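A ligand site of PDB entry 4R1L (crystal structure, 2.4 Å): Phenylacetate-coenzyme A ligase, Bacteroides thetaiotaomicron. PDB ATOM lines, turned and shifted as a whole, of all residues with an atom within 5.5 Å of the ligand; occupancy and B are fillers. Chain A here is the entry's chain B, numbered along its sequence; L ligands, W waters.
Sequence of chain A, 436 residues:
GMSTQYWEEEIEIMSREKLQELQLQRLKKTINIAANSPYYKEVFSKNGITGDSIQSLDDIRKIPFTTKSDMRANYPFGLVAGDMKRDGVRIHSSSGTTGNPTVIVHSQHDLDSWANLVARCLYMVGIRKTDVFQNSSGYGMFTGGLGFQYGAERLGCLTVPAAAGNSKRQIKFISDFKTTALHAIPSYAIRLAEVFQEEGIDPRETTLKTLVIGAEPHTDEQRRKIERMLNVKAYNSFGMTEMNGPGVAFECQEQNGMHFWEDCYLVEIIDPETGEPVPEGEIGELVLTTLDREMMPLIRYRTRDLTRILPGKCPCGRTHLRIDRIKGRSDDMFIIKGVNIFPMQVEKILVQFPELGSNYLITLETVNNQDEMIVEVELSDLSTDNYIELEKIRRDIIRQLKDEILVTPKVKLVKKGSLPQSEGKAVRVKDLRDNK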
ATOM      1  N   SER A  94      13.138 -28.266   1.455  1.00  0.00           N
ATOM      2  CA  SER A  94      14.558 -28.134   1.098  1.00  0.00           C
ATOM      3  C   SER A  94      14.765 -26.958   0.143  1.00  0.00           C
ATOM      4  O   SER A  94      13.803 -26.488  -0.474  1.00  0.00           O
ATOM      5  CB  SER A  94      15.086 -29.429   0.472  1.00  0.00           C
ATOM      6  OG  SER A  94      14.316 -29.893  -0.624  1.00  0.00           O
ATOM      7  N   PHE A 142      12.958 -23.409   6.528  1.00  0.00           N
ATOM      8  CA  PHE A 142      14.356 -23.861   6.665  1.00  0.00           C
ATOM      9  C   PHE A 142      14.516 -24.655   7.929  1.00  0.00           C
ATOM     10  O   PHE A 142      14.214 -24.165   8.999  1.00  0.00           O
ATOM     11  CB  PHE A 142      15.354 -22.668   6.663  1.00  0.00           C
ATOM     12  CG  PHE A 142      15.333 -21.804   5.422  1.00  0.00           C
ATOM     13  CD1 PHE A 142      15.761 -22.312   4.192  1.00  0.00           C
ATOM     14  CD2 PHE A 142      14.921 -20.470   5.480  1.00  0.00           C
ATOM     15  CE1 PHE A 142      15.701 -21.531   3.032  1.00  0.00           C
ATOM     16  CE2 PHE A 142      14.895 -19.674   4.326  1.00  0.00           C
ATOM     17  CZ  PHE A 142      15.280 -20.213   3.103  1.00  0.00           C
ATOM     18  N   THR A 143      15.037 -25.887   7.813  1.00  0.00           N
ATOM     19  CA  THR A 143      15.174 -26.789   8.957  1.00  0.00           C
ATOM     20  C   THR A 143      16.217 -26.301   9.999  1.00  0.00           C
ATOM     21  O   THR A 143      16.119 -26.712  11.150  1.00  0.00           O
ATOM     22  CB  THR A 143      15.544 -28.191   8.475  1.00  0.00           C
ATOM     23  OG1 THR A 143      16.841 -28.153   7.913  1.00  0.00           O
ATOM     24  CG2 THR A 143      14.541 -28.767   7.498  1.00  0.00           C
ATOM     25  N   GLY A 144      17.199 -25.475   9.596  1.00  0.00           N
ATOM     26  CA  GLY A 144      18.218 -24.944  10.495  1.00  0.00           C
ATOM     27  C   GLY A 144      17.689 -24.046  11.598  1.00  0.00           C
ATOM     28  O   GLY A 144      18.255 -24.001  12.696  1.00  0.00           O
ATOM     29  N   ILE A 213      29.190 -24.717  12.479  1.00  0.00           N
ATOM     30  CA  ILE A 213      29.145 -24.278  11.065  1.00  0.00           C
ATOM     31  C   ILE A 213      28.792 -25.477  10.150  1.00  0.00           C
ATOM     32  O   ILE A 213      29.382 -26.554  10.266  1.00  0.00           O
ATOM     33  CB  ILE A 213      30.484 -23.596  10.626  1.00  0.00           C
ATOM     34  CG1 ILE A 213      31.706 -24.536  10.820  1.00  0.00           C
ATOM     35  CG2 ILE A 213      30.673 -22.237  11.359  1.00  0.00           C
ATOM     36  CD1 ILE A 213      33.072 -23.979  10.370  1.00  0.00           C
ATOM     37  N   GLY A 214      27.835 -25.251   9.251  1.00  0.00           N
ATOM     38  CA  GLY A 214      27.399 -26.262   8.287  1.00  0.00           C
ATOM     39  C   GLY A 214      26.874 -25.671   6.999  1.00  0.00           C
ATOM     40  O   GLY A 214      27.216 -24.530   6.661  1.00  0.00           O
ATOM     41  N   ALA A 215      26.019 -26.436   6.268  1.00  0.00           N
ATOM     42  CA  ALA A 215      25.328 -26.092   5.015  1.00  0.00           C
ATOM     43  C   ALA A 215      26.282 -25.952   3.808  1.00  0.00           C
ATOM     44  O   ALA A 215      25.955 -26.428   2.738  1.00  0.00           O
ATOM     45  CB  ALA A 215      24.540 -24.796   5.158  1.00  0.00           C
ATOM     46  N   GLU A 216      27.428 -25.245   3.967  1.00  0.00           N
ATOM     47  CA  GLU A 216      28.409 -24.994   2.909  1.00  0.00           C
ATOM     48  C   GLU A 216      29.634 -25.922   2.941  1.00  0.00           C
ATOM     49  O   GLU A 216      30.305 -25.987   3.970  1.00  0.00           O
ATOM     50  CB  GLU A 216      28.964 -23.554   3.042  1.00  0.00           C
ATOM     51  CG  GLU A 216      28.039 -22.365   2.822  1.00  0.00           C
ATOM     52  CD  GLU A 216      28.691 -21.022   3.117  1.00  0.00           C
ATOM     53  OE1 GLU A 216      29.658 -20.984   3.912  1.00  0.00           O
ATOM     54  OE2 GLU A 216      28.217 -20.005   2.574  1.00  0.00           O
ATOM     55  N   PRO A 217      30.063 -26.525   1.801  1.00  0.00           N
ATOM     56  CA  PRO A 217      31.361 -27.206   1.805  1.00  0.00           C
ATOM     57  C   PRO A 217      32.475 -26.198   2.111  1.00  0.00           C
ATOM     58  O   PRO A 217      32.443 -25.045   1.631  1.00  0.00           O
ATOM     59  CB  PRO A 217      31.485 -27.775   0.384  1.00  0.00           C
ATOM     60  CG  PRO A 217      30.073 -27.762  -0.158  1.00  0.00           C
ATOM     61  CD  PRO A 217      29.451 -26.541   0.452  1.00  0.00           C
ATOM     62  N   HIS A 218      33.428 -26.597   2.945  1.00  0.00           N
ATOM     63  CA  HIS A 218      34.530 -25.725   3.334  1.00  0.00           C
ATOM     64  C   HIS A 218      35.669 -26.581   3.749  1.00  0.00           C
ATOM     65  O   HIS A 218      35.445 -27.691   4.246  1.00  0.00           O
ATOM     66  CB  HIS A 218      34.120 -24.733   4.449  1.00  0.00           C
ATOM     67  CG  HIS A 218      33.647 -25.406   5.704  1.00  0.00           C
ATOM     68  ND1 HIS A 218      32.352 -25.911   5.812  1.00  0.00           N
ATOM     69  CD2 HIS A 218      34.319 -25.682   6.842  1.00  0.00           C
ATOM     70  CE1 HIS A 218      32.284 -26.463   7.013  1.00  0.00           C
ATOM     71  NE2 HIS A 218      33.427 -26.327   7.684  1.00  0.00           N
ATOM     72  N   ASN A 236      32.104 -28.785  12.556  1.00  0.00           N
ATOM     73  CA  ASN A 236      31.395 -29.092  11.330  1.00  0.00           C
ATOM     74  C   ASN A 236      30.085 -29.817  11.670  1.00  0.00           C
ATOM     75  O   ASN A 236      30.080 -30.777  12.438  1.00  0.00           O
ATOM     76  CB  ASN A 236      32.274 -29.927  10.375  1.00  0.00           C
ATOM     77  CG  ASN A 236      31.880 -29.797   8.915  1.00  0.00           C
ATOM     78  OD1 ASN A 236      30.925 -29.083   8.558  1.00  0.00           O
ATOM     79  ND2 ASN A 236      32.629 -30.468   8.047  1.00  0.00           N
ATOM     80  N   SER A 237      29.000 -29.284  11.128  1.00  0.00           N
ATOM     81  CA  SER A 237      27.613 -29.711  11.297  1.00  0.00           C
ATOM     82  C   SER A 237      26.996 -30.148   9.975  1.00  0.00           C
ATOM     83  O   SER A 237      26.874 -29.345   9.039  1.00  0.00           O
ATOM     84  CB  SER A 237      26.793 -28.560  11.888  1.00  0.00           C
ATOM     85  OG  SER A 237      25.403 -28.893  11.948  1.00  0.00           O
ATOM     86  N   PHE A 238      26.622 -31.434   9.894  1.00  0.00           N
ATOM     87  CA  PHE A 238      26.018 -31.948   8.669  1.00  0.00           C
ATOM     88  C   PHE A 238      24.539 -32.185   8.849  1.00  0.00           C
ATOM     89  O   PHE A 238      24.093 -32.692   9.875  1.00  0.00           O
ATOM     90  CB  PHE A 238      26.697 -33.254   8.213  1.00  0.00           C
ATOM     91  CG  PHE A 238      26.156 -33.817   6.926  1.00  0.00           C
ATOM     92  CD1 PHE A 238      26.469 -33.230   5.702  1.00  0.00           C
ATOM     93  CD2 PHE A 238      25.298 -34.918   6.929  1.00  0.00           C
ATOM     94  CE1 PHE A 238      25.931 -33.735   4.500  1.00  0.00           C
ATOM     95  CE2 PHE A 238      24.761 -35.422   5.738  1.00  0.00           C
ATOM     96  CZ  PHE A 238      25.089 -34.831   4.532  1.00  0.00           C
ATOM     97  N   GLY A 239      23.810 -31.910   7.796  1.00  0.00           N
ATOM     98  CA  GLY A 239      22.388 -32.178   7.753  1.00  0.00           C
ATOM     99  C   GLY A 239      21.784 -31.916   6.390  1.00  0.00           C
ATOM    100  O   GLY A 239      22.429 -31.322   5.521  1.00  0.00           O
ATOM    101  N   MET A 240      20.548 -32.389   6.218  1.00  0.00           N
ATOM    102  CA  MET A 240      19.722 -32.188   5.049  1.00  0.00           C
ATOM    103  C   MET A 240      18.316 -32.393   5.452  1.00  0.00           C
ATOM    104  O   MET A 240      18.053 -33.223   6.341  1.00  0.00           O
ATOM    105  CB  MET A 240      20.129 -33.089   3.886  1.00  0.00           C
ATOM    106  CG  MET A 240      19.899 -34.574   4.124  1.00  0.00           C
ATOM    107  SD  MET A 240      20.508 -35.609   2.643  1.00  0.00           S
ATOM    108  CE  MET A 240      22.212 -35.762   3.234  1.00  0.00           C
ATOM    109  N   THR A 241      17.408 -31.613   4.834  1.00  0.00           N
ATOM    110  CA  THR A 241      15.964 -31.589   5.089  1.00  0.00           C
ATOM    111  C   THR A 241      15.396 -33.018   5.068  1.00  0.00           C
ATOM    112  O   THR A 241      14.650 -33.377   5.975  1.00  0.00           O
ATOM    113  CB  THR A 241      15.271 -30.694   4.041  1.00  0.00           C
ATOM    114  OG1 THR A 241      15.820 -29.394   4.166  1.00  0.00           O
ATOM    115  CG2 THR A 241      13.747 -30.644   4.210  1.00  0.00           C
ATOM    116  N   GLU A 242      15.797 -33.823   4.058  1.00  0.00           N
ATOM    117  CA  GLU A 242      15.350 -35.203   3.901  1.00  0.00           C
ATOM    118  C   GLU A 242      15.634 -36.042   5.139  1.00  0.00           C
ATOM    119  O   GLU A 242      14.850 -36.945   5.462  1.00  0.00           O
ATOM    120  CB  GLU A 242      16.020 -35.872   2.686  1.00  0.00           C
ATOM    121  CG  GLU A 242      15.618 -35.270   1.347  1.00  0.00           C
ATOM    122  CD  GLU A 242      16.345 -34.002   0.917  1.00  0.00           C
ATOM    123  OE1 GLU A 242      17.151 -33.449   1.701  1.00  0.00           O
ATOM    124  OE2 GLU A 242      16.082 -33.566  -0.217  1.00  0.00           O
ATOM    125  N   GLY A 245      17.041 -32.356   9.087  1.00  0.00           N
ATOM    126  CA  GLY A 245      17.720 -31.081   8.931  1.00  0.00           C
ATOM    127  C   GLY A 245      19.049 -31.196   9.650  1.00  0.00           C
ATOM    128  O   GLY A 245      19.758 -32.182   9.416  1.00  0.00           O
ATOM    129  N   MET A 258      33.023 -36.484  11.002  1.00  0.00           N
ATOM    130  CA  MET A 258      31.709 -36.212  11.579  1.00  0.00           C
ATOM    131  C   MET A 258      31.029 -37.515  11.968  1.00  0.00           C
ATOM    132  O   MET A 258      30.758 -38.342  11.105  1.00  0.00           O
ATOM    133  CB  MET A 258      30.844 -35.403  10.592  1.00  0.00           C
ATOM    134  CG  MET A 258      31.293 -33.969  10.451  1.00  0.00           C
ATOM    135  SD  MET A 258      30.197 -32.957   9.284  1.00  0.00           S
ATOM    136  CE  MET A 258      30.818 -33.701   7.556  1.00  0.00           C
ATOM    137  N   THR A 303      21.718 -39.155  -1.770  1.00  0.00           N
ATOM    138  CA  THR A 303      21.871 -37.766  -1.328  1.00  0.00           C
ATOM    139  C   THR A 303      22.527 -36.831  -2.348  1.00  0.00           C
ATOM    140  O   THR A 303      22.318 -35.608  -2.256  1.00  0.00           O
ATOM    141  CB  THR A 303      22.694 -37.713  -0.050  1.00  0.00           C
ATOM    142  OG1 THR A 303      24.013 -38.218  -0.314  1.00  0.00           O
ATOM    143  CG2 THR A 303      22.038 -38.466   1.085  1.00  0.00           C
ATOM    144  N   ASP A 305      25.604 -36.411  -2.311  1.00  0.00           N
ATOM    145  CA  ASP A 305      26.772 -35.958  -1.558  1.00  0.00           C
ATOM    146  C   ASP A 305      27.857 -36.991  -1.637  1.00  0.00           C
ATOM    147  O   ASP A 305      27.625 -38.179  -1.395  1.00  0.00           O
ATOM    148  CB  ASP A 305      26.434 -35.654  -0.097  1.00  0.00           C
ATOM    149  CG  ASP A 305      25.482 -34.508   0.102  1.00  0.00           C
ATOM    150  OD1 ASP A 305      25.639 -33.479  -0.594  1.00  0.00           O
ATOM    151  OD2 ASP A 305      24.555 -34.646   0.934  1.00  0.00           O
ATOM    152  N   ILE A 326      32.438 -33.135   3.480  1.00  0.00           N
ATOM    153  CA  ILE A 326      31.743 -33.360   2.216  1.00  0.00           C
ATOM    154  C   ILE A 326      32.558 -32.694   1.096  1.00  0.00           C
ATOM    155  O   ILE A 326      32.779 -31.478   1.103  1.00  0.00           O
ATOM    156  CB  ILE A 326      30.255 -32.907   2.196  1.00  0.00           C
ATOM    157  CG1 ILE A 326      29.415 -33.594   3.320  1.00  0.00           C
ATOM    158  CG2 ILE A 326      29.607 -33.071   0.823  1.00  0.00           C
ATOM    159  CD1 ILE A 326      29.146 -35.089   3.230  1.00  0.00           C
ATOM    160  N   GLY A 328      31.659 -32.380  -1.930  1.00  0.00           N
ATOM    161  CA  GLY A 328      30.655 -31.545  -2.586  1.00  0.00           C
ATOM    162  C   GLY A 328      29.436 -32.357  -2.981  1.00  0.00           C
ATOM    163  O   GLY A 328      29.356 -33.566  -2.719  1.00  0.00           O
ATOM    164  N   ARG A 329      28.462 -31.682  -3.626  1.00  0.00           N
ATOM    165  CA  ARG A 329      27.249 -32.291  -4.160  1.00  0.00           C
ATOM    166  C   ARG A 329      27.440 -32.450  -5.662  1.00  0.00           C
ATOM    167  O   ARG A 329      28.091 -31.596  -6.251  1.00  0.00           O
ATOM    168  CB  ARG A 329      25.991 -31.469  -3.817  1.00  0.00           C
ATOM    169  CG  ARG A 329      24.718 -32.306  -3.863  1.00  0.00           C
ATOM    170  CD  ARG A 329      23.485 -31.500  -3.521  1.00  0.00           C
ATOM    171  NE  ARG A 329      22.762 -32.005  -2.362  1.00  0.00           N
ATOM    172  CZ  ARG A 329      21.605 -31.494  -1.920  1.00  0.00           C
ATOM    173  NH1 ARG A 329      21.028 -30.487  -2.575  1.00  0.00           N
ATOM    174  NH2 ARG A 329      21.019 -32.001  -0.842  1.00  0.00           N
ATOM    175  N   LYS A 425      23.666 -19.756   1.470  1.00  0.00           N
ATOM    176  CA  LYS A 425      24.870 -20.452   1.020  1.00  0.00           C
ATOM    177  C   LYS A 425      25.550 -19.646  -0.051  1.00  0.00           C
ATOM    178  O   LYS A 425      24.873 -19.198  -0.992  1.00  0.00           O
ATOM    179  CB  LYS A 425      24.554 -21.872   0.483  1.00  0.00           C
ATOM    180  CG  LYS A 425      23.955 -22.847   1.462  1.00  0.00           C
ATOM    181  CD  LYS A 425      23.880 -24.237   0.853  1.00  0.00           C
ATOM    182  CE  LYS A 425      23.091 -25.152   1.752  1.00  0.00           C
ATOM    183  NZ  LYS A 425      23.260 -26.578   1.388  1.00  0.00           N
HETATM  184  P1  LIG L   1      19.834 -26.581   4.625  1.00  0.00           P
HETATM  185  O1  LIG L   1      19.929 -27.641   5.727  1.00  0.00           O
HETATM  186  O2  LIG L   1      21.189 -25.899   4.346  1.00  0.00           O
HETATM  187  O3  LIG L   1      18.754 -25.511   4.902  1.00  0.00           O
HETATM  188  P2  LIG L   1      19.319 -28.629   2.579  1.00  0.00           P
HETATM  189  O4  LIG L   1      18.651 -29.597   3.471  1.00  0.00           O
HETATM  190  O5  LIG L   1      18.488 -28.508   1.316  1.00  0.00           O
HETATM  191  O6  LIG L   1      19.354 -27.173   3.225  1.00  0.00           O
HETATM  192  O7  LIG L   1      20.848 -28.888   2.206  1.00  0.00           O
HETATM  193  C1  LIG L   1      21.534 -30.086   2.576  1.00  0.00           C
HETATM  194  C2  LIG L   1      22.798 -30.203   1.769  1.00  0.00           C
HETATM  195  O8  LIG L   1      23.744 -29.186   2.159  1.00  0.00           O
HETATM  196  C3  LIG L   1      23.541 -31.510   1.943  1.00  0.00           C
HETATM  197  O9  LIG L   1      22.957 -32.536   1.153  1.00  0.00           O
HETATM  198  C4  LIG L   1      24.953 -31.124   1.504  1.00  0.00           C
HETATM  199  O10 LIG L   1      25.114 -31.110   0.090  1.00  0.00           O
HETATM  200  C5  LIG L   1      25.066 -29.712   2.097  1.00  0.00           C
HETATM  201  N1  LIG L   1      25.665 -29.679   3.426  1.00  0.00           N
HETATM  202  C6  LIG L   1      25.029 -29.650   4.632  1.00  0.00           C
HETATM  203  N2  LIG L   1      25.838 -29.610   5.671  1.00  0.00           N
HETATM  204  C7  LIG L   1      27.102 -29.624   5.097  1.00  0.00           C
HETATM  205  C8  LIG L   1      28.401 -29.612   5.656  1.00  0.00           C
HETATM  206  N3  LIG L   1      28.642 -29.547   6.970  1.00  0.00           N
HETATM  207  N4  LIG L   1      29.450 -29.637   4.798  1.00  0.00           N
HETATM  208  C9  LIG L   1      29.217 -29.671   3.490  1.00  0.00           C
HETATM  209  N5  LIG L   1      28.036 -29.698   2.843  1.00  0.00           N
HETATM  210  C10 LIG L   1      27.011 -29.674   3.709  1.00  0.00           C
HETATM  211  O   HOH W   1      21.480 -28.971   7.519  1.00  0.00           O
HETATM  212  O   HOH W   2      16.276 -26.839   4.875  1.00  0.00           O
HETATM  213  O   HOH W   3      18.283 -24.194   7.162  1.00  0.00           O
HETATM  214  O   HOH W   4      31.932 -30.717   5.043  1.00  0.00           O
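OD1 of Asn 236 sits at hydrogen-bond distance from N3 of the ligand (2.8 Å). An oxygen (O4) of the ligand lies within hydrogen-bond range of the side-chain hydroxyl of Thr 241 (2.9 Å). NH2 of Arg 329 is in hydrogen-bond range of O9 of the ligand (2.8 Å). A nitrogen (N2) of the ligand is in hydrogen-bond range of the backbone NH (N) of Ala 215 (3.2 Å). An oxygen (O10) of the ligand lies within hydrogen-bond range of the side-chain carboxylate of Asp 305 (2.5 Å). O4 of the ligand sits at hydrogen-bond distance from N of Thr 241, 2.7 Å away. N3 of the ligand is in hydrogen-bond range of O of Ser 237 (2.7 Å). The side-chain amino group (NZ) of Lys 425 lies within salt-bridge range of an oxygen (O2) of the ligand (3.7 Å).
The backbone carbonyl oxygen (O) of Ala 215 is in hydrogen-bond range of the side-chain amino group (NZ) of Lys 425. OD1 of Asn 236 sits close to O of Ile 213 (3.4 Å). N of Asp 305 sits close to OG1 of Thr 303, 3.1 Å away. SD of Met 258 lies close to ND2 of Asn 236 (3.7 Å). O of Met 240 is in hydrogen-bond range of N of Gly 245, 3.1 Å away. The side-chain carboxylate (OD1) of Asp 305 is in salt-bridge range of the guanidinium group (NE) of Arg 329 (3.7 Å). The backbone NH (N) of Ser 237 sits at hydrogen-bond distance from the backbone carbonyl oxygen (O) of Ile 213, at 2.9 Å. A ring nitrogen (ND1) of His 218 lies within hydrogen-bond range of the backbone carbonyl oxygen of Glu 216 (2.8 Å).
Ser 94 touches the ligand. Thr 143 touches the ligand (OG1 to O1, 3.8 Å). CA of Gly 214 touches N3 of the ligand, 3.8 Å away. Glu 216 touches the ligand (C to C9, 3.8 Å). Pro 217 touches the ligand (N to C9, 3.7 Å). CD1 of Phe 238 touches N2 of the ligand (3.7 Å). O of Gly 239 touches C6 of the ligand (3.2 Å). Met 240 touches the ligand (CA to O4, 3.2 Å). Ile 326 touches the ligand (CB to C9, 3.6 Å). Of the 25 residues printed, 16 come within 4 Å of the ligand. The nearest printed residue that does not touch the ligand is Met 258 (4.4 Å).
Water W3 bridges an oxygen (O3) of the ligand and the backbone NH of Gly 144. Water W1 lies within hydrogen-bond range of an oxygen (O1) of the ligand (2.7 Å) and the backbone carbonyl oxygen (O) of Gly 239 (3.2 Å). Water W4 lies within hydrogen-bond range of N4 of the ligand (2.7 Å), N of Ile 326 (2.9 Å) and ND2 of Asn 236 (3.1 Å). Water W2 lies within hydrogen-bond range of OG1 of Thr 241 (2.7 Å), O3 of the ligand (2.8 Å) and N of Thr 143 (3.3 Å).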
